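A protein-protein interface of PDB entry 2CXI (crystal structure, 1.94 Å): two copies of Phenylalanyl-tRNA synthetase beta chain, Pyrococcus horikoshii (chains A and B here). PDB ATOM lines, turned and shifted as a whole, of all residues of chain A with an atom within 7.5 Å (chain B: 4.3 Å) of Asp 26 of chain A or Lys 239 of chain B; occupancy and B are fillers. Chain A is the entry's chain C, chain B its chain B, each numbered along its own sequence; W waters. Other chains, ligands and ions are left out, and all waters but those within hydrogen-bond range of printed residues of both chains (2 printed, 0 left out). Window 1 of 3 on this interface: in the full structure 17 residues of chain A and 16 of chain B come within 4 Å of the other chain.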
ATOM      1  N   SER A  20      26.970 -21.633   5.228  1.00  0.00           N
ATOM      2  CA  SER A  20      25.718 -22.304   4.902  1.00  0.00           C
ATOM      3  C   SER A  20      24.553 -21.530   5.549  1.00  0.00           C
ATOM      4  O   SER A  20      24.759 -20.745   6.488  1.00  0.00           O
ATOM      5  CB  SER A  20      25.740 -23.743   5.450  1.00  0.00           C
ATOM      6  OG  SER A  20      25.697 -23.684   6.871  1.00  0.00           O
ATOM      7  N   ILE A  21      23.346 -21.753   5.039  1.00  0.00           N
ATOM      8  CA  ILE A  21      22.145 -21.194   5.655  1.00  0.00           C
ATOM      9  C   ILE A  21      22.040 -21.625   7.113  1.00  0.00           C
ATOM     10  O   ILE A  21      21.682 -20.820   7.970  1.00  0.00           O
ATOM     11  CB  ILE A  21      20.900 -21.599   4.836  1.00  0.00           C
ATOM     12  CG1 ILE A  21      20.970 -20.988   3.422  1.00  0.00           C
ATOM     13  CG2 ILE A  21      19.580 -21.219   5.539  1.00  0.00           C
ATOM     14  CD1 ILE A  21      20.979 -19.468   3.403  1.00  0.00           C
ATOM     15  N   GLU A  22      22.364 -22.889   7.389  1.00  0.00           N
ATOM     16  CA  GLU A  22      22.372 -23.400   8.765  1.00  0.00           C
ATOM     17  C   GLU A  22      23.337 -22.580   9.630  1.00  0.00           C
ATOM     18  O   GLU A  22      22.994 -22.180  10.734  1.00  0.00           O
ATOM     19  CB  GLU A  22      22.672 -24.907   8.811  1.00  0.00           C
ATOM     20  CG  GLU A  22      22.567 -25.484  10.228  1.00  0.00           C
ATOM     21  CD  GLU A  22      22.871 -26.974  10.350  1.00  0.00           C
ATOM     22  OE1 GLU A  22      22.770 -27.697   9.342  1.00  0.00           O
ATOM     23  OE2 GLU A  22      23.202 -27.412  11.476  1.00  0.00           O
ATOM     24  N   GLU A  23      24.529 -22.277   9.115  1.00  0.00           N
ATOM     25  CA  GLU A  23      25.440 -21.381   9.838  1.00  0.00           C
ATOM     26  C   GLU A  23      24.955 -19.941   9.951  1.00  0.00           C
ATOM     27  O   GLU A  23      25.191 -19.316  10.983  1.00  0.00           O
ATOM     28  CB  GLU A  23      26.821 -21.372   9.216  1.00  0.00           C
ATOM     29  CG  GLU A  23      27.525 -22.694   9.279  1.00  0.00           C
ATOM     30  CD  GLU A  23      28.844 -22.671   8.501  1.00  0.00           C
ATOM     31  OE1 GLU A  23      28.863 -22.281   7.304  1.00  0.00           O
ATOM     32  OE2 GLU A  23      29.852 -23.067   9.103  1.00  0.00           O
ATOM     33  N   TRP A  24      24.284 -19.430   8.915  1.00  0.00           N
ATOM     34  CA  TRP A  24      23.724 -18.077   8.929  1.00  0.00           C
ATOM     35  C   TRP A  24      22.696 -17.860  10.030  1.00  0.00           C
ATOM     36  O   TRP A  24      22.535 -16.750  10.534  1.00  0.00           O
ATOM     37  CB  TRP A  24      23.139 -17.704   7.571  1.00  0.00           C
ATOM     38  CG  TRP A  24      24.169 -17.004   6.740  1.00  0.00           C
ATOM     39  CD1 TRP A  24      24.830 -17.502   5.654  1.00  0.00           C
ATOM     40  CD2 TRP A  24      24.681 -15.671   6.955  1.00  0.00           C
ATOM     41  NE1 TRP A  24      25.709 -16.553   5.166  1.00  0.00           N
ATOM     42  CE2 TRP A  24      25.648 -15.431   5.962  1.00  0.00           C
ATOM     43  CE3 TRP A  24      24.419 -14.659   7.903  1.00  0.00           C
ATOM     44  CZ2 TRP A  24      26.354 -14.205   5.870  1.00  0.00           C
ATOM     45  CZ3 TRP A  24      25.105 -13.473   7.833  1.00  0.00           C
ATOM     46  CH2 TRP A  24      26.066 -13.241   6.811  1.00  0.00           C
ATOM     47  N   GLU A  25      22.030 -18.932  10.426  1.00  0.00           N
ATOM     48  CA  GLU A  25      21.201 -18.928  11.674  1.00  0.00           C
ATOM     49  C   GLU A  25      21.907 -18.385  12.896  1.00  0.00           C
ATOM     50  O   GLU A  25      21.342 -17.609  13.650  1.00  0.00           O
ATOM     51  CB  GLU A  25      20.775 -20.368  12.007  1.00  0.00           C
ATOM     52  CG  GLU A  25      19.822 -20.962  11.002  1.00  0.00           C
ATOM     53  CD  GLU A  25      18.463 -20.326  11.053  1.00  0.00           C
ATOM     54  OE1 GLU A  25      18.118 -19.661  12.060  1.00  0.00           O
ATOM     55  OE2 GLU A  25      17.735 -20.502  10.067  1.00  0.00           O
ATOM     56  N   ASP A  26      23.139 -18.812  13.109  1.00  0.00           N
ATOM     57  CA  ASP A  26      23.909 -18.364  14.260  1.00  0.00           C
ATOM     58  C   ASP A  26      24.519 -16.973  14.036  1.00  0.00           C
ATOM     59  O   ASP A  26      24.562 -16.146  14.955  1.00  0.00           O
ATOM     60  CB  ASP A  26      25.026 -19.364  14.543  1.00  0.00           C
ATOM     61  CG  ASP A  26      24.502 -20.720  15.001  1.00  0.00           C
ATOM     62  OD1 ASP A  26      23.408 -20.766  15.594  1.00  0.00           O
ATOM     63  OD2 ASP A  26      25.136 -21.780  14.769  1.00  0.00           O
ATOM     64  N   LEU A  27      25.032 -16.743  12.818  1.00  0.00           N
ATOM     65  CA  LEU A  27      25.738 -15.497  12.493  1.00  0.00           C
ATOM     66  C   LEU A  27      24.908 -14.215  12.656  1.00  0.00           C
ATOM     67  O   LEU A  27      25.414 -13.205  13.159  1.00  0.00           O
ATOM     68  CB  LEU A  27      26.283 -15.565  11.064  1.00  0.00           C
ATOM     69  CG  LEU A  27      27.394 -16.564  10.745  1.00  0.00           C
ATOM     70  CD1 LEU A  27      27.671 -16.443   9.225  1.00  0.00           C
ATOM     71  CD2 LEU A  27      28.664 -16.278  11.562  1.00  0.00           C
ATOM     72  N   VAL A  28      23.645 -14.241  12.251  1.00  0.00           N
ATOM     73  CA  VAL A  28      22.797 -13.038  12.373  1.00  0.00           C
ATOM     74  C   VAL A  28      22.667 -12.613  13.831  1.00  0.00           C
ATOM     75  O   VAL A  28      22.483 -11.435  14.116  1.00  0.00           O
ATOM     76  CB  VAL A  28      21.396 -13.201  11.708  1.00  0.00           C
ATOM     77  CG1 VAL A  28      21.555 -13.467  10.205  1.00  0.00           C
ATOM     78  CG2 VAL A  28      20.603 -14.317  12.351  1.00  0.00           C
ATOM     79  N   LEU A  29      22.791 -13.571  14.742  1.00  0.00           N
ATOM     80  CA  LEU A  29      22.675 -13.261  16.174  1.00  0.00           C
ATOM     81  C   LEU A  29      23.852 -12.390  16.635  1.00  0.00           C
ATOM     82  O   LEU A  29      23.693 -11.535  17.528  1.00  0.00           O
ATOM     83  CB  LEU A  29      22.542 -14.549  17.003  1.00  0.00           C
ATOM     84  CG  LEU A  29      21.294 -15.397  16.671  1.00  0.00           C
ATOM     85  CD1 LEU A  29      21.245 -16.789  17.384  1.00  0.00           C
ATOM     86  CD2 LEU A  29      19.936 -14.633  16.841  1.00  0.00           C
ATOM     87  N   TYR A  30      25.007 -12.568  15.981  1.00  0.00           N
ATOM     88  CA  TYR A  30      26.185 -11.753  16.245  1.00  0.00           C
ATOM     89  C   TYR A  30      25.998 -10.300  15.864  1.00  0.00           C
ATOM     90  O   TYR A  30      26.666  -9.417  16.424  1.00  0.00           O
ATOM     91  CB  TYR A  30      27.432 -12.277  15.519  1.00  0.00           C
ATOM     92  CG  TYR A  30      27.849 -13.649  15.881  1.00  0.00           C
ATOM     93  CD1 TYR A  30      27.465 -14.210  17.092  1.00  0.00           C
ATOM     94  CD2 TYR A  30      28.648 -14.412  15.010  1.00  0.00           C
ATOM     95  CE1 TYR A  30      27.847 -15.497  17.444  1.00  0.00           C
ATOM     96  CE2 TYR A  30      29.033 -15.703  15.357  1.00  0.00           C
ATOM     97  CZ  TYR A  30      28.634 -16.229  16.581  1.00  0.00           C
ATOM     98  OH  TYR A  30      28.985 -17.490  16.965  1.00  0.00           O
ATOM     99  N   ALA A  31      25.104 -10.042  14.912  1.00  0.00           N
ATOM    100  CA  ALA A  31      24.844  -8.687  14.447  1.00  0.00           C
ATOM    101  C   ALA A  31      23.591  -8.131  15.135  1.00  0.00           C
ATOM    102  O   ALA A  31      23.042  -7.117  14.708  1.00  0.00           O
ATOM    103  CB  ALA A  31      24.669  -8.686  12.916  1.00  0.00           C
ATOM    104  N   CYS A  33      20.611  -9.364  15.198  1.00  0.00           N
ATOM    105  CA  CYS A  33      19.501  -9.471  14.245  1.00  0.00           C
ATOM    106  C   CYS A  33      18.881 -10.854  14.391  1.00  0.00           C
ATOM    107  O   CYS A  33      19.528 -11.785  14.893  1.00  0.00           O
ATOM    108  CB  CYS A  33      20.038  -9.300  12.820  1.00  0.00           C
ATOM    109  SG  CYS A  33      20.403  -7.579  12.444  1.00  0.00           S
ATOM    110  N   LEU A  35      16.814 -13.707  11.786  1.00  0.00           N
ATOM    111  CA  LEU A  35      16.586 -14.004  10.383  1.00  0.00           C
ATOM    112  C   LEU A  35      15.104 -14.107  10.167  1.00  0.00           C
ATOM    113  O   LEU A  35      14.492 -15.134  10.519  1.00  0.00           O
ATOM    114  CB  LEU A  35      17.206 -15.339  10.019  1.00  0.00           C
ATOM    115  CG  LEU A  35      18.024 -15.435   8.756  1.00  0.00           C
ATOM    116  CD1 LEU A  35      18.336 -16.900   8.462  1.00  0.00           C
ATOM    117  CD2 LEU A  35      17.430 -14.691   7.570  1.00  0.00           C
ATOM    118  N   ILE A  69      29.746  -9.094  12.304  1.00  0.00           N
ATOM    119  CA  ILE A  69      30.095 -10.513  12.166  1.00  0.00           C
ATOM    120  C   ILE A  69      31.603 -10.693  12.034  1.00  0.00           C
ATOM    121  O   ILE A  69      32.154 -11.589  12.677  1.00  0.00           O
ATOM    122  CB  ILE A  69      29.301 -11.165  10.990  1.00  0.00           C
ATOM    123  CG1 ILE A  69      27.797 -11.262  11.382  1.00  0.00           C
ATOM    124  CG2 ILE A  69      29.910 -12.522  10.561  1.00  0.00           C
ATOM    125  CD1 ILE A  69      26.865 -11.460  10.169  1.00  0.00           C
ATOM    126  N   TYR B 103      16.761 -30.647  10.149  1.00  0.00           N
ATOM    127  CA  TYR B 103      16.515 -31.395  11.379  1.00  0.00           C
ATOM    128  C   TYR B 103      15.075 -31.820  11.569  1.00  0.00           C
ATOM    129  O   TYR B 103      14.176 -31.038  11.350  1.00  0.00           O
ATOM    130  CB  TYR B 103      16.982 -30.597  12.619  1.00  0.00           C
ATOM    131  CG  TYR B 103      18.444 -30.336  12.545  1.00  0.00           C
ATOM    132  CD1 TYR B 103      19.370 -31.367  12.781  1.00  0.00           C
ATOM    133  CD2 TYR B 103      18.926 -29.078  12.186  1.00  0.00           C
ATOM    134  CE1 TYR B 103      20.763 -31.130  12.678  1.00  0.00           C
ATOM    135  CE2 TYR B 103      20.326 -28.835  12.085  1.00  0.00           C
ATOM    136  CZ  TYR B 103      21.227 -29.876  12.314  1.00  0.00           C
ATOM    137  OH  TYR B 103      22.620 -29.666  12.207  1.00  0.00           O
ATOM    138  N   GLY B 237      13.163 -28.086  11.526  1.00  0.00           N
ATOM    139  CA  GLY B 237      13.727 -26.755  11.459  1.00  0.00           C
ATOM    140  C   GLY B 237      15.198 -26.784  11.091  1.00  0.00           C
ATOM    141  O   GLY B 237      15.700 -27.755  10.515  1.00  0.00           O
ATOM    142  N   TRP B 238      15.888 -25.710  11.456  1.00  0.00           N
ATOM    143  CA  TRP B 238      17.280 -25.460  11.020  1.00  0.00           C
ATOM    144  C   TRP B 238      18.290 -25.587  12.138  1.00  0.00           C
ATOM    145  O   TRP B 238      19.519 -25.596  11.886  1.00  0.00           O
ATOM    146  CB  TRP B 238      17.330 -24.053  10.394  1.00  0.00           C
ATOM    147  CG  TRP B 238      16.790 -24.077   9.006  1.00  0.00           C
ATOM    148  CD1 TRP B 238      15.494 -23.844   8.600  1.00  0.00           C
ATOM    149  CD2 TRP B 238      17.533 -24.378   7.814  1.00  0.00           C
ATOM    150  NE1 TRP B 238      15.401 -23.964   7.230  1.00  0.00           N
ATOM    151  CE2 TRP B 238      16.633 -24.297   6.721  1.00  0.00           C
ATOM    152  CE3 TRP B 238      18.871 -24.711   7.563  1.00  0.00           C
ATOM    153  CZ2 TRP B 238      17.030 -24.549   5.389  1.00  0.00           C
ATOM    154  CZ3 TRP B 238      19.269 -24.971   6.249  1.00  0.00           C
ATOM    155  CH2 TRP B 238      18.348 -24.877   5.174  1.00  0.00           C
ATOM    156  N   LYS B 239      17.806 -25.685  13.373  1.00  0.00           N
ATOM    157  CA  LYS B 239      18.710 -25.786  14.542  1.00  0.00           C
ATOM    158  C   LYS B 239      18.196 -26.867  15.496  1.00  0.00           C
ATOM    159  O   LYS B 239      17.048 -26.782  15.977  1.00  0.00           O
ATOM    160  CB  LYS B 239      18.842 -24.451  15.311  1.00  0.00           C
ATOM    161  CG  LYS B 239      19.416 -23.233  14.555  1.00  0.00           C
ATOM    162  CD  LYS B 239      20.725 -23.541  13.729  1.00  0.00           C
ATOM    163  CE  LYS B 239      22.028 -23.431  14.522  1.00  0.00           C
ATOM    164  NZ  LYS B 239      23.255 -23.399  13.615  1.00  0.00           N
ATOM    165  N   LEU B 240      19.056 -27.830  15.827  1.00  0.00           N
ATOM    166  CA  LEU B 240      18.638 -28.962  16.616  1.00  0.00           C
ATOM    167  C   LEU B 240      18.132 -28.513  17.992  1.00  0.00           C
ATOM    168  O   LEU B 240      17.112 -29.007  18.435  1.00  0.00           O
ATOM    169  CB  LEU B 240      19.729 -30.025  16.727  1.00  0.00           C
ATOM    170  CG  LEU B 240      19.403 -31.336  17.413  1.00  0.00           C
ATOM    171  CD1 LEU B 240      18.252 -32.091  16.665  1.00  0.00           C
ATOM    172  CD2 LEU B 240      20.661 -32.235  17.566  1.00  0.00           C
ATOM    173  N   GLU B 241      18.803 -27.553  18.644  1.00  0.00           N
ATOM    174  CA  GLU B 241      18.345 -27.145  19.981  1.00  0.00           C
ATOM    175  C   GLU B 241      16.992 -26.465  19.938  1.00  0.00           C
ATOM    176  O   GLU B 241      16.226 -26.572  20.903  1.00  0.00           O
ATOM    177  CB  GLU B 241      19.387 -26.319  20.793  1.00  0.00           C
ATOM    178  CG  GLU B 241      19.312 -24.786  20.763  1.00  0.00           C
ATOM    179  CD  GLU B 241      18.122 -24.081  21.482  1.00  0.00           C
ATOM    180  OE1 GLU B 241      17.645 -24.454  22.604  1.00  0.00           O
ATOM    181  OE2 GLU B 241      17.647 -23.093  20.892  1.00  0.00           O
ATOM    182  N   LYS B 242      16.701 -25.738  18.863  1.00  0.00           N
ATOM    183  CA  LYS B 242      15.378 -25.085  18.774  1.00  0.00           C
ATOM    184  C   LYS B 242      14.230 -26.077  18.633  1.00  0.00           C
ATOM    185  O   LYS B 242      13.190 -25.949  19.311  1.00  0.00           O
ATOM    186  CB  LYS B 242      15.278 -24.095  17.629  1.00  0.00           C
ATOM    187  CG  LYS B 242      16.088 -22.844  17.842  1.00  0.00           C
ATOM    188  CD  LYS B 242      15.394 -21.634  17.241  1.00  0.00           C
ATOM    189  CE  LYS B 242      14.301 -21.125  18.139  1.00  0.00           C
ATOM    190  NZ  LYS B 242      13.886 -19.731  17.811  1.00  0.00           N
ATOM    191  N   VAL B 243      14.410 -27.028  17.737  1.00  0.00           N
ATOM    192  CA  VAL B 243      13.344 -28.021  17.494  1.00  0.00           C
ATOM    193  C   VAL B 243      13.170 -28.911  18.724  1.00  0.00           C
ATOM    194  O   VAL B 243      12.051 -29.330  19.026  1.00  0.00           O
ATOM    195  CB  VAL B 243      13.567 -28.827  16.179  1.00  0.00           C
ATOM    196  CG1 VAL B 243      13.460 -27.899  14.929  1.00  0.00           C
ATOM    197  CG2 VAL B 243      14.891 -29.596  16.175  1.00  0.00           C
HETATM  198  O   HOH W   1      16.722 -20.854   7.033  1.00  0.00           O
HETATM  199  O   HOH W   2      23.610 -26.092  13.761  1.00  0.00           O
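Printed residues of chain B within 4 Å of Ile 21 of chain A: Trp 238.
Of the printed residues of chain B, Glu 22 of chain A touches Tyr 103, Trp 238 and Lys 239.
Trp 24 of chain A touches none of the printed residues of chain B.
Of the printed residues of chain B, Glu 25 of chain A touches Trp 238 and Lys 239.
Asp 26 of chain A touches one residue of chain B.
Of the printed residues of chain A, Tyr 103 of chain B touches Glu 22.
Printed residues of chain A within 4 Å of Trp 238 of chain B: Ile 21, Glu 22 and Glu 25.
Lys 239 of chain B touches three residues of chain A.
The nearest printed residue of chain B that does not touch Asp 26 of chain A is Trp 238 of chain B (7.2 Å).
The backbone NH (N) of Tyr 103 of chain B is in hydrogen-bond range of the backbone carbonyl oxygen (O) of Gly 237 of chain B (3.1 Å).
The side-chain hydroxyl (OG) of Ser 20 of chain A lies close to the backbone NH (N) of Glu 22 of chain A (3.5 Å).
Ile 21 of chain A touches Trp 238 of chain B (CG2 to CZ3, 3.8 Å).
Trp 238 of chain B touches Glu 22 of chain A.
OE2 of Glu 25 of chain A touches CB of Trp 238 of chain B (3.6 Å).
Lys 239 of chain B touches Glu 25 of chain A (CD to CB, 3.6 Å).
Water W2 bridges OE2 of Glu 22 of chain A (2.7 Å) and NZ of Lys 239 of chain B (2.7 Å).
Water W1 bridges OE2 of Glu 25 of chain A (3.2 Å) and NE1 of Trp 238 of chain B (3.4 Å).
No position is printed for both chains.
Of the 7 pairs that touch across the chains among the printed residues, none has its exchanged pair printed and touching as well.
The backbone carbonyl oxygen (O) of Glu 22 of chain A is in hydrogen-bond range of the side-chain amino group (NZ) of Lys 239 of chain B (3.1 Å).
OH of Tyr 103 of chain B sits at hydrogen-bond distance from OE2 of Glu 22 of chain A (2.4 Å).
NZ of Lys 239 of chain B lies within salt-bridge range of OD2 of Asp 26 of chain A (2.7 Å).
Hydrophobic or aromatic side chains of chain A within 4 Å of the printed part of chain B: Ile 21.
Of the 8 printed residues of chain B, 3 touch a printed residue of chain A.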
